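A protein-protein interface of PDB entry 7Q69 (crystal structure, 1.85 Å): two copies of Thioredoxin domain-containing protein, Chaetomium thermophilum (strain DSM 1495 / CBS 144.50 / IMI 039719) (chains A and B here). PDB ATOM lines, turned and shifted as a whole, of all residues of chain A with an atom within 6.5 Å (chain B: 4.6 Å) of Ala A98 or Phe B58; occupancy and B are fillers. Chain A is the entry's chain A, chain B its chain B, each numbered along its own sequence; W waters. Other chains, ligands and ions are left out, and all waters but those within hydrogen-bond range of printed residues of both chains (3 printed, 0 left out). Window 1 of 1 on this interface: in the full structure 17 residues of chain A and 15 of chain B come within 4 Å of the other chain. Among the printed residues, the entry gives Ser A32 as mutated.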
ATOM      1  N   ILE A  21      -0.867   0.006   7.659  1.00  0.00           N
ATOM      2  CA  ILE A  21       0.187   1.010   7.710  1.00  0.00           C
ATOM      3  C   ILE A  21      -0.106   1.916   8.907  1.00  0.00           C
ATOM      4  O   ILE A  21      -1.151   2.593   8.944  1.00  0.00           O
ATOM      5  CB  ILE A  21       0.272   1.798   6.397  1.00  0.00           C
ATOM      6  CG1 ILE A  21       0.589   0.826   5.249  1.00  0.00           C
ATOM      7  CG2 ILE A  21       1.329   2.875   6.501  1.00  0.00           C
ATOM      8  CD1 ILE A  21       0.405   1.370   3.915  1.00  0.00           C
ATOM      9  N   LEU A  29      -1.154  11.999   1.495  1.00  0.00           N
ATOM     10  CA  LEU A  29      -1.574  10.797   0.778  1.00  0.00           C
ATOM     11  C   LEU A  29      -0.476  10.201  -0.103  1.00  0.00           C
ATOM     12  O   LEU A  29      -0.562   9.022  -0.473  1.00  0.00           O
ATOM     13  CB  LEU A  29      -2.787  11.118  -0.098  1.00  0.00           C
ATOM     14  CG  LEU A  29      -4.101  11.424   0.624  1.00  0.00           C
ATOM     15  CD1 LEU A  29      -4.948  12.361  -0.211  1.00  0.00           C
ATOM     16  CD2 LEU A  29      -4.813  10.119   0.889  1.00  0.00           C
ATOM     17  N   THR A  30       0.532  10.984  -0.461  1.00  0.00           N
ATOM     18  CA  THR A  30       1.602  10.524  -1.334  1.00  0.00           C
ATOM     19  C   THR A  30       2.734   9.836  -0.579  1.00  0.00           C
ATOM     20  O   THR A  30       3.716   9.422  -1.203  1.00  0.00           O
ATOM     21  CB  THR A  30       2.173  11.692  -2.150  1.00  0.00           C
ATOM     22  OG1 THR A  30       2.859  12.623  -1.304  1.00  0.00           O
ATOM     23  CG2 THR A  30       1.047  12.426  -2.897  1.00  0.00           C
ATOM     24  N   VAL A  31       2.629   9.702   0.734  1.00  0.00           N
ATOM     25  CA  VAL A  31       3.571   8.923   1.526  1.00  0.00           C
ATOM     26  C   VAL A  31       2.916   7.568   1.739  1.00  0.00           C
ATOM     27  O   VAL A  31       1.949   7.458   2.499  1.00  0.00           O
ATOM     28  CB  VAL A  31       3.905   9.605   2.859  1.00  0.00           C
ATOM     29  CG1 VAL A  31       4.873   8.745   3.671  1.00  0.00           C
ATOM     30  CG2 VAL A  31       4.509  10.968   2.607  1.00  0.00           C
ATOM     31  N   SER A  32       3.419   6.539   1.047  1.00  0.00           N
ATOM     32  CA  SER A  32       2.703   5.265   0.987  1.00  0.00           C
ATOM     33  C   SER A  32       2.843   4.460   2.274  1.00  0.00           C
ATOM     34  O   SER A  32       1.852   3.896   2.753  1.00  0.00           O
ATOM     35  CB  SER A  32       3.189   4.443  -0.210  1.00  0.00           C
ATOM     36  OG  SER A  32       2.967   5.157  -1.420  1.00  0.00           O
ATOM     37  N   GLY A  33       4.048   4.403   2.848  1.00  0.00           N
ATOM     38  CA  GLY A  33       4.281   3.627   4.058  1.00  0.00           C
ATOM     39  C   GLY A  33       4.702   2.187   3.784  1.00  0.00           C
ATOM     40  O   GLY A  33       4.989   1.773   2.658  1.00  0.00           O
ATOM     41  N   PHE A  58     -13.436   3.686  -0.214  1.00  0.00           N
ATOM     42  CA  PHE A  58     -13.783   4.686  -1.217  1.00  0.00           C
ATOM     43  C   PHE A  58     -15.081   4.401  -1.964  1.00  0.00           C
ATOM     44  O   PHE A  58     -15.404   5.123  -2.882  1.00  0.00           O
ATOM     45  CB  PHE A  58     -12.647   4.861  -2.234  1.00  0.00           C
ATOM     46  CG  PHE A  58     -11.394   5.451  -1.646  1.00  0.00           C
ATOM     47  CD1 PHE A  58     -11.349   6.780  -1.259  1.00  0.00           C
ATOM     48  CD2 PHE A  58     -10.264   4.668  -1.476  1.00  0.00           C
ATOM     49  CE1 PHE A  58     -10.191   7.328  -0.699  1.00  0.00           C
ATOM     50  CE2 PHE A  58      -9.097   5.212  -0.922  1.00  0.00           C
ATOM     51  CZ  PHE A  58      -9.079   6.547  -0.538  1.00  0.00           C
ATOM     52  N   ASP A  92      -6.103  -3.627   0.147  1.00  0.00           N
ATOM     53  CA  ASP A  92      -4.798  -3.797   0.766  1.00  0.00           C
ATOM     54  C   ASP A  92      -4.494  -2.646   1.740  1.00  0.00           C
ATOM     55  O   ASP A  92      -5.205  -1.627   1.808  1.00  0.00           O
ATOM     56  CB  ASP A  92      -3.708  -3.927  -0.296  1.00  0.00           C
ATOM     57  CG  ASP A  92      -3.556  -2.693  -1.159  1.00  0.00           C
ATOM     58  OD1 ASP A  92      -3.321  -1.612  -0.618  1.00  0.00           O
ATOM     59  OD2 ASP A  92      -3.621  -2.827  -2.395  1.00  0.00           O
ATOM     60  N   ALA A  93      -3.411  -2.826   2.509  1.00  0.00           N
ATOM     61  CA  ALA A  93      -3.080  -1.860   3.551  1.00  0.00           C
ATOM     62  C   ALA A  93      -2.818  -0.474   2.977  1.00  0.00           C
ATOM     63  O   ALA A  93      -3.118   0.536   3.627  1.00  0.00           O
ATOM     64  CB  ALA A  93      -1.859  -2.336   4.326  1.00  0.00           C
ATOM     65  N   PHE A  94      -2.259  -0.395   1.764  1.00  0.00           N
ATOM     66  CA  PHE A  94      -1.971   0.922   1.196  1.00  0.00           C
ATOM     67  C   PHE A  94      -3.260   1.677   0.893  1.00  0.00           C
ATOM     68  O   PHE A  94      -3.359   2.889   1.128  1.00  0.00           O
ATOM     69  CB  PHE A  94      -1.113   0.780  -0.061  1.00  0.00           C
ATOM     70  CG  PHE A  94       0.209   0.081   0.175  1.00  0.00           C
ATOM     71  CD1 PHE A  94       1.294   0.775   0.682  1.00  0.00           C
ATOM     72  CD2 PHE A  94       0.349  -1.256  -0.106  1.00  0.00           C
ATOM     73  CE1 PHE A  94       2.503   0.151   0.888  1.00  0.00           C
ATOM     74  CE2 PHE A  94       1.570  -1.900   0.092  1.00  0.00           C
ATOM     75  CZ  PHE A  94       2.632  -1.195   0.609  1.00  0.00           C
ATOM     76  N   VAL A  95      -4.235   0.984   0.315  1.00  0.00           N
ATOM     77  CA  VAL A  95      -5.497   1.622  -0.017  1.00  0.00           C
ATOM     78  C   VAL A  95      -6.227   2.010   1.248  1.00  0.00           C
ATOM     79  O   VAL A  95      -6.802   3.102   1.325  1.00  0.00           O
ATOM     80  CB  VAL A  95      -6.354   0.700  -0.897  1.00  0.00           C
ATOM     81  CG1 VAL A  95      -7.746   1.279  -1.089  1.00  0.00           C
ATOM     82  CG2 VAL A  95      -5.650   0.491  -2.290  1.00  0.00           C
ATOM     83  N   MET A  96      -6.202   1.129   2.266  1.00  0.00           N
ATOM     84  CA  MET A  96      -6.876   1.421   3.528  1.00  0.00           C
ATOM     85  C   MET A  96      -6.252   2.623   4.226  1.00  0.00           C
ATOM     86  O   MET A  96      -6.968   3.467   4.772  1.00  0.00           O
ATOM     87  CB  MET A  96      -6.831   0.198   4.443  1.00  0.00           C
ATOM     88  CG  MET A  96      -7.690  -0.944   3.993  1.00  0.00           C
ATOM     89  SD  MET A  96      -9.430  -0.587   3.774  1.00  0.00           S
ATOM     90  CE  MET A  96      -9.975  -0.337   5.506  1.00  0.00           C
ATOM     91  N   SER A  97      -4.923   2.739   4.174  1.00  0.00           N
ATOM     92  CA  SER A  97      -4.236   3.893   4.746  1.00  0.00           C
ATOM     93  C   SER A  97      -4.659   5.184   4.054  1.00  0.00           C
ATOM     94  O   SER A  97      -4.955   6.188   4.713  1.00  0.00           O
ATOM     95  CB  SER A  97      -2.725   3.687   4.640  1.00  0.00           C
ATOM     96  OG  SER A  97      -2.028   4.822   5.104  1.00  0.00           O
ATOM     97  N   ALA A  98      -4.719   5.167   2.719  1.00  0.00           N
ATOM     98  CA  ALA A  98      -5.173   6.340   1.983  1.00  0.00           C
ATOM     99  C   ALA A  98      -6.608   6.699   2.355  1.00  0.00           C
ATOM    100  O   ALA A  98      -6.967   7.878   2.444  1.00  0.00           O
ATOM    101  CB  ALA A  98      -5.039   6.089   0.477  1.00  0.00           C
ATOM    102  N   TRP A  99      -7.453   5.694   2.550  1.00  0.00           N
ATOM    103  CA  TRP A  99      -8.848   5.968   2.865  1.00  0.00           C
ATOM    104  C   TRP A  99      -8.974   6.664   4.219  1.00  0.00           C
ATOM    105  O   TRP A  99      -9.763   7.612   4.367  1.00  0.00           O
ATOM    106  CB  TRP A  99      -9.642   4.660   2.827  1.00  0.00           C
ATOM    107  CG  TRP A  99     -11.119   4.837   2.892  1.00  0.00           C
ATOM    108  CD1 TRP A  99     -11.859   5.800   2.286  1.00  0.00           C
ATOM    109  CD2 TRP A  99     -12.036   4.035   3.645  1.00  0.00           C
ATOM    110  NE1 TRP A  99     -13.194   5.632   2.591  1.00  0.00           N
ATOM    111  CE2 TRP A  99     -13.325   4.557   3.427  1.00  0.00           C
ATOM    112  CE3 TRP A  99     -11.885   2.927   4.492  1.00  0.00           C
ATOM    113  CZ2 TRP A  99     -14.460   4.025   4.041  1.00  0.00           C
ATOM    114  CZ3 TRP A  99     -13.005   2.385   5.081  1.00  0.00           C
ATOM    115  CH2 TRP A  99     -14.281   2.948   4.869  1.00  0.00           C
ATOM    116  N   GLY A 100      -8.219   6.203   5.223  1.00  0.00           N
ATOM    117  CA  GLY A 100      -8.244   6.876   6.513  1.00  0.00           C
ATOM    118  C   GLY A 100      -7.739   8.304   6.419  1.00  0.00           C
ATOM    119  O   GLY A 100      -8.321   9.226   7.006  1.00  0.00           O
ATOM    120  N   LYS A 101      -6.660   8.511   5.659  1.00  0.00           N
ATOM    121  CA  LYS A 101      -6.124   9.860   5.510  1.00  0.00           C
ATOM    122  C   LYS A 101      -7.107  10.743   4.758  1.00  0.00           C
ATOM    123  O   LYS A 101      -7.263  11.924   5.081  1.00  0.00           O
ATOM    124  CB  LYS A 101      -4.775   9.831   4.797  1.00  0.00           C
ATOM    125  CG  LYS A 101      -3.617   9.333   5.671  1.00  0.00           C
ATOM    126  CD  LYS A 101      -2.320   9.428   4.921  1.00  0.00           C
ATOM    127  CE  LYS A 101      -1.683   8.073   4.689  1.00  0.00           C
ATOM    128  NZ  LYS A 101      -0.391   8.208   3.974  1.00  0.00           N
ATOM    129  N   ALA A 102      -7.766  10.183   3.738  1.00  0.00           N
ATOM    130  CA  ALA A 102      -8.781  10.929   2.994  1.00  0.00           C
ATOM    131  C   ALA A 102      -9.896  11.410   3.912  1.00  0.00           C
ATOM    132  O   ALA A 102     -10.521  12.446   3.653  1.00  0.00           O
ATOM    133  CB  ALA A 102      -9.348  10.056   1.874  1.00  0.00           C
ATOM    134  N   ASN A 103     -10.166  10.667   4.977  1.00  0.00           N
ATOM    135  CA  ASN A 103     -11.158  11.047   5.970  1.00  0.00           C
ATOM    136  C   ASN A 103     -10.582  11.823   7.140  1.00  0.00           C
ATOM    137  O   ASN A 103     -11.256  11.955   8.172  1.00  0.00           O
ATOM    138  CB  ASN A 103     -11.862   9.799   6.480  1.00  0.00           C
ATOM    139  CG  ASN A 103     -12.924   9.317   5.507  1.00  0.00           C
ATOM    140  OD1 ASN A 103     -14.043   9.825   5.515  1.00  0.00           O
ATOM    141  ND2 ASN A 103     -12.568   8.373   4.635  1.00  0.00           N
ATOM    142  N   GLY B  56      -0.601  -1.821  -8.181  1.00  0.00           N
ATOM    143  CA  GLY B  56      -1.621  -1.329  -7.273  1.00  0.00           C
ATOM    144  C   GLY B  56      -1.648   0.168  -7.043  1.00  0.00           C
ATOM    145  O   GLY B  56      -0.599   0.794  -6.852  1.00  0.00           O
ATOM    146  N   ALA B  57      -2.842   0.758  -7.063  1.00  0.00           N
ATOM    147  CA  ALA B  57      -2.981   2.132  -6.616  1.00  0.00           C
ATOM    148  C   ALA B  57      -2.423   2.284  -5.206  1.00  0.00           C
ATOM    149  O   ALA B  57      -2.537   1.384  -4.375  1.00  0.00           O
ATOM    150  CB  ALA B  57      -4.449   2.561  -6.652  1.00  0.00           C
ATOM    151  N   PHE B  58      -1.829   3.442  -4.937  1.00  0.00           N
ATOM    152  CA  PHE B  58      -1.314   3.863  -3.635  1.00  0.00           C
ATOM    153  C   PHE B  58      -0.147   3.014  -3.131  1.00  0.00           C
ATOM    154  O   PHE B  58       0.302   3.230  -2.007  1.00  0.00           O
ATOM    155  CB  PHE B  58      -2.405   3.878  -2.546  1.00  0.00           C
ATOM    156  CG  PHE B  58      -3.471   4.917  -2.755  1.00  0.00           C
ATOM    157  CD1 PHE B  58      -3.211   6.243  -2.493  1.00  0.00           C
ATOM    158  CD2 PHE B  58      -4.723   4.571  -3.255  1.00  0.00           C
ATOM    159  CE1 PHE B  58      -4.190   7.211  -2.691  1.00  0.00           C
ATOM    160  CE2 PHE B  58      -5.701   5.527  -3.453  1.00  0.00           C
ATOM    161  CZ  PHE B  58      -5.433   6.854  -3.159  1.00  0.00           C
ATOM    162  N   THR B  59       0.379   2.077  -3.919  1.00  0.00           N
ATOM    163  CA  THR B  59       1.534   1.317  -3.453  1.00  0.00           C
ATOM    164  C   THR B  59       2.814   2.107  -3.704  1.00  0.00           C
ATOM    165  O   THR B  59       2.845   2.998  -4.560  1.00  0.00           O
ATOM    166  CB  THR B  59       1.617  -0.036  -4.155  1.00  0.00           C
ATOM    167  OG1 THR B  59       1.726   0.156  -5.574  1.00  0.00           O
ATOM    168  CG2 THR B  59       0.374  -0.869  -3.837  1.00  0.00           C
ATOM    169  N   PRO B  60       3.897   1.774  -2.988  1.00  0.00           N
ATOM    170  CA  PRO B  60       5.046   2.703  -2.930  1.00  0.00           C
ATOM    171  C   PRO B  60       5.682   3.020  -4.274  1.00  0.00           C
ATOM    172  O   PRO B  60       5.843   4.198  -4.619  1.00  0.00           O
ATOM    173  CB  PRO B  60       6.036   1.978  -2.005  1.00  0.00           C
ATOM    174  CG  PRO B  60       5.165   1.059  -1.151  1.00  0.00           C
ATOM    175  CD  PRO B  60       4.067   0.606  -2.097  1.00  0.00           C
ATOM    176  N   GLN B  63       3.197   4.832  -6.599  1.00  0.00           N
ATOM    177  CA  GLN B  63       2.895   6.196  -6.183  1.00  0.00           C
ATOM    178  C   GLN B  63       4.133   7.080  -6.265  1.00  0.00           C
ATOM    179  O   GLN B  63       4.155   8.078  -6.990  1.00  0.00           O
ATOM    180  CB  GLN B  63       2.327   6.199  -4.756  1.00  0.00           C
ATOM    181  CG  GLN B  63       2.192   7.592  -4.158  1.00  0.00           C
ATOM    182  CD  GLN B  63       1.294   8.483  -4.994  1.00  0.00           C
ATOM    183  OE1 GLN B  63       0.238   8.047  -5.489  1.00  0.00           O
ATOM    184  NE2 GLN B  63       1.715   9.736  -5.178  1.00  0.00           N
ATOM    185  N   VAL B  95     -11.428   3.213  -6.144  1.00  0.00           N
ATOM    186  CA  VAL B  95     -10.068   3.368  -5.653  1.00  0.00           C
ATOM    187  C   VAL B  95      -9.211   4.096  -6.678  1.00  0.00           C
ATOM    188  O   VAL B  95      -8.413   4.977  -6.321  1.00  0.00           O
ATOM    189  CB  VAL B  95      -9.483   1.993  -5.285  1.00  0.00           C
ATOM    190  CG1 VAL B  95      -8.013   2.126  -4.883  1.00  0.00           C
ATOM    191  CG2 VAL B  95     -10.302   1.355  -4.153  1.00  0.00           C
ATOM    192  N   ALA B  98      -9.951   7.818  -6.620  1.00  0.00           N
ATOM    193  CA  ALA B  98      -9.348   8.486  -5.483  1.00  0.00           C
ATOM    194  C   ALA B  98      -7.842   8.615  -5.657  1.00  0.00           C
ATOM    195  O   ALA B  98      -7.255   9.594  -5.184  1.00  0.00           O
ATOM    196  CB  ALA B  98      -9.679   7.732  -4.197  1.00  0.00           C
ATOM    197  N   TRP B  99      -7.198   7.629  -6.298  1.00  0.00           N
ATOM    198  CA  TRP B  99      -5.749   7.685  -6.500  1.00  0.00           C
ATOM    199  C   TRP B  99      -5.381   8.830  -7.446  1.00  0.00           C
ATOM    200  O   TRP B  99      -4.423   9.573  -7.190  1.00  0.00           O
ATOM    201  CB  TRP B  99      -5.247   6.325  -7.019  1.00  0.00           C
ATOM    202  CG  TRP B  99      -3.758   6.195  -7.073  1.00  0.00           C
ATOM    203  CD1 TRP B  99      -2.846   6.651  -6.135  1.00  0.00           C
ATOM    204  CD2 TRP B  99      -2.986   5.583  -8.111  1.00  0.00           C
ATOM    205  NE1 TRP B  99      -1.562   6.353  -6.540  1.00  0.00           N
ATOM    206  CE2 TRP B  99      -1.623   5.710  -7.752  1.00  0.00           C
ATOM    207  CE3 TRP B  99      -3.308   4.938  -9.316  1.00  0.00           C
ATOM    208  CZ2 TRP B  99      -0.599   5.222  -8.559  1.00  0.00           C
ATOM    209  CZ3 TRP B  99      -2.290   4.465 -10.100  1.00  0.00           C
ATOM    210  CH2 TRP B  99      -0.956   4.605  -9.721  1.00  0.00           C
ATOM    211  N   ALA B 102      -5.782  11.983  -5.395  1.00  0.00           N
ATOM    212  CA  ALA B 102      -4.676  12.101  -4.454  1.00  0.00           C
ATOM    213  C   ALA B 102      -3.449  12.706  -5.116  1.00  0.00           C
ATOM    214  O   ALA B 102      -2.611  13.321  -4.441  1.00  0.00           O
ATOM    215  CB  ALA B 102      -4.326  10.726  -3.882  1.00  0.00           C
HETATM  216  O   HOH W   1      -3.265  -1.309  -4.407  1.00  0.00           O
HETATM  217  O   HOH W   2       4.437  10.367  -4.265  1.00  0.00           O
HETATM  218  O   HOH W   3       0.204   6.022  -1.469  1.00  0.00           O
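The side-chain hydroxyl (OG) of Ser A32 lies within hydrogen-bond range of the backbone carbonyl oxygen (O) of Phe B58 (3.3 Å).
OD1 of Asp A92 sits at hydrogen-bond distance from N of Phe A94, 2.9 Å away. N of Val A95 lies within hydrogen-bond range of OD1 of Asp A92 (2.9 Å). The backbone carbonyl oxygen of Gly B56 lies within hydrogen-bond range of the side-chain hydroxyl of Thr B59, at 2.7 Å. OE1 of Gln B63 lies within hydrogen-bond range of NE1 of Trp B99, at 2.7 Å.
Among the printed residues, merely in contact across the chains: Thr A30 with Gln B63, Ser A32 with Thr B59, Ser A32 with Pro B60, Ser A32 with Gln B63, Gly A33 with Pro B60, Phe A58 with Ala B98, Phe A94 with Phe B58, Phe A94 with Thr B59, Phe A94 with Pro B60, Val A95 with Ala B57, Val A95 with Val B95 and Ala A98 with Phe B58.
Ile A21 touches none of the printed residues of chain B. Of the printed residues of chain B, Ser A32 touches Phe B58, Thr B59, Pro B60 and Gln B63. Trp A99 touches none of the printed residues of chain B. Of the printed residues of chain A, Ala B57 touches Val A95 (3.9 Å). Of the printed residues of chain A, Gln B63 touches Thr A30 (3.6 Å) and Ser A32 (3.6 Å). Printed residues of chain A within 4 Å of Val B95: Val A95 (3.9 Å). The nearest printed residue of chain B that does not touch Ala A98 is Ala B102 (6.4 Å). The nearest printed residue of chain B that does not touch Val A95 is Phe B58 (4.3 Å).
Of the 10 printed residues of chain B, 7 touch a printed residue of chain A. Of the 19 printed residues of chain A, 7 touch a printed residue of chain B. Printed residues of chain A that touch a printed residue of chain B: Thr A30, Ser A32, Gly A33, Phe A58, Phe A94, Val A95 and Ala A98. Hydrophobic or aromatic side chains of chain A within 4 Å of the printed part of chain B: Phe A58, Phe A94, Val A95 and Ala A98. Among the printed residues, 13 pairs touch across the chains. Among the printed residues, no Asp or Glu carboxylate lies within 4 Å of a Lys or Arg side-chain nitrogen of the other chain.
Phe A58 touches Ala B98, and with the chains exchanged Ala A98 touches Phe B58. Val A95 touches its own counterpart, Val B95. Positions printed for both chains: 58, 95, 98, 99 and 102.
Water W1 bridges the side-chain carboxylate (OD2) of Asp A92 and the backbone carbonyl oxygen (O) of Ala B57. Water W3 lies within hydrogen-bond range of the backbone carbonyl oxygen of Phe B58, the side-chain hydroxyl of Ser A32 and the backbone carbonyl oxygen of Leu A29. Water W2 lies within hydrogen-bond range of the side-chain amide nitrogen (NE2) of Gln B63 (2.9 Å) and the backbone carbonyl oxygen (O) of Thr A30 (3.3 Å).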
